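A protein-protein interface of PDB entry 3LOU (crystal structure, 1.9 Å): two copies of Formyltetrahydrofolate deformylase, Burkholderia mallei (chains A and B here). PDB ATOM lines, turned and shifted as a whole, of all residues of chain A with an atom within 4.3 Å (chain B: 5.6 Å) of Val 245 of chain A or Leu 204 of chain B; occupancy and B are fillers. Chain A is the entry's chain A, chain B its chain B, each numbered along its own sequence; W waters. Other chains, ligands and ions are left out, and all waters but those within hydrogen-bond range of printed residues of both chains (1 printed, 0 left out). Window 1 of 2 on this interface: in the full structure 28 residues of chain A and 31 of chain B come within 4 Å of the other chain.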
ATOM      1  N   SER A 202       9.571  24.612  31.902  1.00  0.00           N
ATOM      2  CA  SER A 202       9.627  24.602  30.445  1.00  0.00           C
ATOM      3  C   SER A 202      10.114  23.259  29.972  1.00  0.00           C
ATOM      4  O   SER A 202      11.050  22.679  30.549  1.00  0.00           O
ATOM      5  CB  SER A 202      10.593  25.646  29.945  1.00  0.00           C
ATOM      6  OG  SER A 202      10.137  26.941  30.224  1.00  0.00           O
ATOM      7  N   PHE A 203       9.485  22.759  28.924  1.00  0.00           N
ATOM      8  CA  PHE A 203       9.787  21.431  28.428  1.00  0.00           C
ATOM      9  C   PHE A 203      10.078  21.439  26.949  1.00  0.00           C
ATOM     10  O   PHE A 203       9.603  22.314  26.209  1.00  0.00           O
ATOM     11  CB  PHE A 203       8.579  20.502  28.675  1.00  0.00           C
ATOM     12  CG  PHE A 203       8.239  20.308  30.124  1.00  0.00           C
ATOM     13  CD1 PHE A 203       8.890  19.351  30.874  1.00  0.00           C
ATOM     14  CD2 PHE A 203       7.240  21.072  30.735  1.00  0.00           C
ATOM     15  CE1 PHE A 203       8.586  19.169  32.214  1.00  0.00           C
ATOM     16  CE2 PHE A 203       6.940  20.891  32.063  1.00  0.00           C
ATOM     17  CZ  PHE A 203       7.617  19.917  32.808  1.00  0.00           C
ATOM     18  N   LEU A 204      10.868  20.453  26.530  1.00  0.00           N
ATOM     19  CA  LEU A 204      11.142  20.196  25.142  1.00  0.00           C
ATOM     20  C   LEU A 204      10.762  18.742  24.845  1.00  0.00           C
ATOM     21  O   LEU A 204      11.391  17.828  25.382  1.00  0.00           O
ATOM     22  CB  LEU A 204      12.619  20.409  24.864  1.00  0.00           C
ATOM     23  CG  LEU A 204      13.034  20.027  23.466  1.00  0.00           C
ATOM     24  CD1 LEU A 204      12.126  20.738  22.498  1.00  0.00           C
ATOM     25  CD2 LEU A 204      14.504  20.345  23.221  1.00  0.00           C
ATOM     26  N   ILE A 224      15.192  19.074  31.055  1.00  0.00           N
ATOM     27  CA  ILE A 224      14.104  19.722  31.836  1.00  0.00           C
ATOM     28  C   ILE A 224      14.503  21.180  31.998  1.00  0.00           C
ATOM     29  O   ILE A 224      15.636  21.470  32.346  1.00  0.00           O
ATOM     30  CB  ILE A 224      13.886  19.077  33.242  1.00  0.00           C
ATOM     31  CG1 ILE A 224      13.433  17.628  33.128  1.00  0.00           C
ATOM     32  CG2 ILE A 224      12.838  19.894  34.067  1.00  0.00           C
ATOM     33  CD1 ILE A 224      12.006  17.478  32.530  1.00  0.00           C
ATOM     34  N   GLY A 225      13.591  22.105  31.732  1.00  0.00           N
ATOM     35  CA  GLY A 225      13.946  23.534  31.772  1.00  0.00           C
ATOM     36  C   GLY A 225      13.025  24.416  32.610  1.00  0.00           C
ATOM     37  O   GLY A 225      12.042  23.952  33.229  1.00  0.00           O
ATOM     38  N   GLN A 243      16.359  31.543  30.418  1.00  0.00           N
ATOM     39  CA  GLN A 243      15.998  30.131  30.228  1.00  0.00           C
ATOM     40  C   GLN A 243      17.186  29.306  30.596  1.00  0.00           C
ATOM     41  O   GLN A 243      18.343  29.670  30.310  1.00  0.00           O
ATOM     42  CB  GLN A 243      15.580  29.813  28.789  1.00  0.00           C
ATOM     43  CG  GLN A 243      14.374  30.580  28.317  1.00  0.00           C
ATOM     44  CD  GLN A 243      14.064  30.341  26.870  1.00  0.00           C
ATOM     45  OE1 GLN A 243      14.895  30.587  25.996  1.00  0.00           O
ATOM     46  NE2 GLN A 243      12.854  29.861  26.596  1.00  0.00           N
ATOM     47  N   VAL A 244      16.924  28.233  31.345  1.00  0.00           N
ATOM     48  CA  VAL A 244      17.952  27.328  31.767  1.00  0.00           C
ATOM     49  C   VAL A 244      17.374  25.899  31.615  1.00  0.00           C
ATOM     50  O   VAL A 244      16.188  25.700  31.817  1.00  0.00           O
ATOM     51  CB  VAL A 244      18.342  27.566  33.249  1.00  0.00           C
ATOM     52  CG1 VAL A 244      19.341  26.496  33.744  1.00  0.00           C
ATOM     53  CG2 VAL A 244      18.854  29.014  33.482  1.00  0.00           C
ATOM     54  N   VAL A 245      18.211  24.937  31.235  1.00  0.00           N
ATOM     55  CA  VAL A 245      17.810  23.532  31.208  1.00  0.00           C
ATOM     56  C   VAL A 245      18.854  22.668  31.936  1.00  0.00           C
ATOM     57  O   VAL A 245      19.999  23.083  32.107  1.00  0.00           O
ATOM     58  CB  VAL A 245      17.625  22.977  29.783  1.00  0.00           C
ATOM     59  CG1 VAL A 245      16.564  23.823  28.984  1.00  0.00           C
ATOM     60  CG2 VAL A 245      18.914  22.925  29.082  1.00  0.00           C
ATOM     61  N   GLU A 246      18.421  21.487  32.367  1.00  0.00           N
ATOM     62  CA  GLU A 246      19.282  20.497  33.027  1.00  0.00           C
ATOM     63  C   GLU A 246      19.053  19.133  32.384  1.00  0.00           C
ATOM     64  O   GLU A 246      17.907  18.750  32.102  1.00  0.00           O
ATOM     65  CB  GLU A 246      18.983  20.418  34.531  1.00  0.00           C
ATOM     66  CG  GLU A 246      19.568  19.154  35.269  1.00  0.00           C
ATOM     67  CD  GLU A 246      21.101  19.060  35.235  1.00  0.00           C
ATOM     68  OE1 GLU A 246      21.757  20.125  35.260  1.00  0.00           O
ATOM     69  OE2 GLU A 246      21.636  17.905  35.200  1.00  0.00           O
ATOM     70  N   SER B 202      14.951  22.130  17.631  1.00  0.00           N
ATOM     71  CA  SER B 202      14.022  22.196  18.746  1.00  0.00           C
ATOM     72  C   SER B 202      14.126  23.514  19.467  1.00  0.00           C
ATOM     73  O   SER B 202      15.232  24.048  19.679  1.00  0.00           O
ATOM     74  CB  SER B 202      14.306  21.094  19.749  1.00  0.00           C
ATOM     75  OG  SER B 202      14.063  19.819  19.196  1.00  0.00           O
ATOM     76  N   PHE B 203      12.990  24.030  19.885  1.00  0.00           N
ATOM     77  CA  PHE B 203      12.972  25.291  20.612  1.00  0.00           C
ATOM     78  C   PHE B 203      12.178  25.231  21.899  1.00  0.00           C
ATOM     79  O   PHE B 203      11.302  24.378  22.068  1.00  0.00           O
ATOM     80  CB  PHE B 203      12.357  26.381  19.732  1.00  0.00           C
ATOM     81  CG  PHE B 203      13.014  26.538  18.409  1.00  0.00           C
ATOM     82  CD1 PHE B 203      14.133  27.343  18.262  1.00  0.00           C
ATOM     83  CD2 PHE B 203      12.478  25.924  17.282  1.00  0.00           C
ATOM     84  CE1 PHE B 203      14.727  27.498  16.992  1.00  0.00           C
ATOM     85  CE2 PHE B 203      13.057  26.056  16.050  1.00  0.00           C
ATOM     86  CZ  PHE B 203      14.171  26.857  15.890  1.00  0.00           C
ATOM     87  N   LEU B 204      12.538  26.124  22.820  1.00  0.00           N
ATOM     88  CA  LEU B 204      11.772  26.334  24.058  1.00  0.00           C
ATOM     89  C   LEU B 204      11.364  27.813  24.122  1.00  0.00           C
ATOM     90  O   LEU B 204      12.205  28.675  24.272  1.00  0.00           O
ATOM     91  CB  LEU B 204      12.561  25.956  25.335  1.00  0.00           C
ATOM     92  CG  LEU B 204      13.034  24.517  25.582  1.00  0.00           C
ATOM     93  CD1 LEU B 204      14.363  24.258  24.870  1.00  0.00           C
ATOM     94  CD2 LEU B 204      13.202  24.248  27.062  1.00  0.00           C
ATOM     95  N   PRO B 205      10.054  28.122  23.901  1.00  0.00           N
ATOM     96  CA  PRO B 205       8.943  27.236  23.545  1.00  0.00           C
ATOM     97  C   PRO B 205       9.064  26.803  22.084  1.00  0.00           C
ATOM     98  O   PRO B 205       9.923  27.334  21.332  1.00  0.00           O
ATOM     99  CB  PRO B 205       7.705  28.125  23.724  1.00  0.00           C
ATOM    100  CG  PRO B 205       8.206  29.506  23.364  1.00  0.00           C
ATOM    101  CD  PRO B 205       9.652  29.541  23.885  1.00  0.00           C
ATOM    102  N   GLY B 206       8.214  25.867  21.675  1.00  0.00           N
ATOM    103  CA  GLY B 206       8.240  25.377  20.320  1.00  0.00           C
ATOM    104  C   GLY B 206       7.734  26.443  19.336  1.00  0.00           C
ATOM    105  O   GLY B 206       6.883  27.261  19.679  1.00  0.00           O
ATOM    106  N   PHE B 207       8.291  26.453  18.134  1.00  0.00           N
ATOM    107  CA  PHE B 207       7.797  27.316  17.060  1.00  0.00           C
ATOM    108  C   PHE B 207       7.421  26.443  15.867  1.00  0.00           C
ATOM    109  O   PHE B 207       8.204  25.593  15.435  1.00  0.00           O
ATOM    110  CB  PHE B 207       8.843  28.343  16.648  1.00  0.00           C
ATOM    111  CG  PHE B 207       9.250  29.226  17.756  1.00  0.00           C
ATOM    112  CD1 PHE B 207       8.358  30.124  18.288  1.00  0.00           C
ATOM    113  CD2 PHE B 207      10.505  29.116  18.318  1.00  0.00           C
ATOM    114  CE1 PHE B 207       8.720  30.898  19.345  1.00  0.00           C
ATOM    115  CE2 PHE B 207      10.863  29.876  19.369  1.00  0.00           C
ATOM    116  CZ  PHE B 207       9.984  30.783  19.884  1.00  0.00           C
ATOM    117  N   VAL B 221      14.382  33.999  22.495  1.00  0.00           N
ATOM    118  CA  VAL B 221      14.746  32.816  23.231  1.00  0.00           C
ATOM    119  C   VAL B 221      16.234  32.916  23.603  1.00  0.00           C
ATOM    120  O   VAL B 221      16.982  33.629  22.961  1.00  0.00           O
ATOM    121  CB  VAL B 221      14.488  31.545  22.437  1.00  0.00           C
ATOM    122  CG1 VAL B 221      12.973  31.417  22.138  1.00  0.00           C
ATOM    123  CG2 VAL B 221      15.338  31.508  21.153  1.00  0.00           C
ATOM    124  N   LEU B 223      17.958  29.995  24.312  1.00  0.00           N
ATOM    125  CA  LEU B 223      18.467  28.659  24.031  1.00  0.00           C
ATOM    126  C   LEU B 223      17.973  28.230  22.652  1.00  0.00           C
ATOM    127  O   LEU B 223      16.902  28.619  22.228  1.00  0.00           O
ATOM    128  CB  LEU B 223      17.976  27.653  25.063  1.00  0.00           C
ATOM    129  CG  LEU B 223      18.269  27.877  26.524  1.00  0.00           C
ATOM    130  CD1 LEU B 223      17.546  26.809  27.340  1.00  0.00           C
ATOM    131  CD2 LEU B 223      19.790  27.872  26.797  1.00  0.00           C
ATOM    132  N   VAL B 245      20.900  21.471  23.739  1.00  0.00           N
ATOM    133  CA  VAL B 245      20.634  22.867  23.539  1.00  0.00           C
ATOM    134  C   VAL B 245      21.921  23.649  23.714  1.00  0.00           C
ATOM    135  O   VAL B 245      22.856  23.180  24.393  1.00  0.00           O
ATOM    136  CB  VAL B 245      19.563  23.430  24.516  1.00  0.00           C
ATOM    137  CG1 VAL B 245      18.213  22.723  24.344  1.00  0.00           C
ATOM    138  CG2 VAL B 245      20.062  23.351  25.955  1.00  0.00           C
HETATM  139  O   HOH W   1       9.332  23.381  23.646  1.00  0.00           O
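The backbone carbonyl oxygen of Leu 204 of chain B is in hydrogen-bond range of the side-chain amide nitrogen of Gln 243 of chain A (2.7 Å).
Water W1 lies within hydrogen-bond range of O of Phe 203 of chain B (2.7 Å), O of Phe 203 of chain A (2.8 Å) and N of Gly 206 of chain B (3.4 Å).
Leu 204 of chain A touches Ser 202 of chain B, but with the chains exchanged Ser 202 of chain A does not touch Leu 204 of chain B (4.1 Å). Leu 204 of chain A touches Phe 203 of chain B, but with the chains exchanged Phe 203 of chain A does not touch Leu 204 of chain B (4.1 Å). Val 245 of chain A touches Leu 204 of chain B, but with the chains exchanged Leu 204 of chain A does not touch Val 245 of chain B (4.5 Å). Val 245 of chain A touches its own counterpart, Val 245 of chain B. Positions printed for both chains: 202, 203, 204 and 245. Of the 8 pairs that touch across the chains among the printed residues, 1 has its exchanged pair printed and touching as well.
Leu 204 of chain A touches Ser 202 of chain B (CD1 to CB, 3.5 Å). CD1 of Leu 204 of chain A touches O of Phe 203 of chain B, 3.8 Å away. OE1 of Gln 243 of chain A touches CA of Val 221 of chain B (3.6 Å). Gln 243 of chain A touches Leu 223 of chain B (OE1 to N, 3.5 Å). Leu 204 of chain B touches Val 245 of chain A (CD2 to CG1, 3.9 Å). Val 245 of chain A touches Leu 223 of chain B (CG1 to CD1, 3.5 Å). CG2 of Val 245 of chain A touches CG2 of Val 245 of chain B, 3.4 Å away.
Of the 9 printed residues of chain A, 3 touch a printed residue of chain B. Hydrophobic or aromatic side chains of chain A that line the printed part of chain B: Leu 204 and Val 245. Of the 9 printed residues of chain B, 6 touch a printed residue of chain A. Hydrophobic or aromatic side chains of chain B that line the printed part of chain A: Leu 204, Val 221, Leu 223 and Val 245. Among the printed residues, no Asp or Glu carboxylate lies within 4 Å of a Lys or Arg side-chain nitrogen of the other chain.
Of the printed residues of chain B, Gln 243 of chain A touches Leu 204, Val 221 and Leu 223. Of the printed residues of chain B, Val 245 of chain A touches Leu 204 (3.9 Å), Leu 223 (3.5 Å) and Val 245 (3.4 Å). Of the printed residues of chain A, Ser 202 of chain B touches Leu 204 (3.5 Å). Of the printed residues of chain A, Phe 203 of chain B touches Leu 204 (3.8 Å). Pro 205 of chain B touches none of the printed residues of chain A. Phe 207 of chain B touches none of the printed residues of chain A. Of the printed residues of chain A, Val 221 of chain B touches Gln 243.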
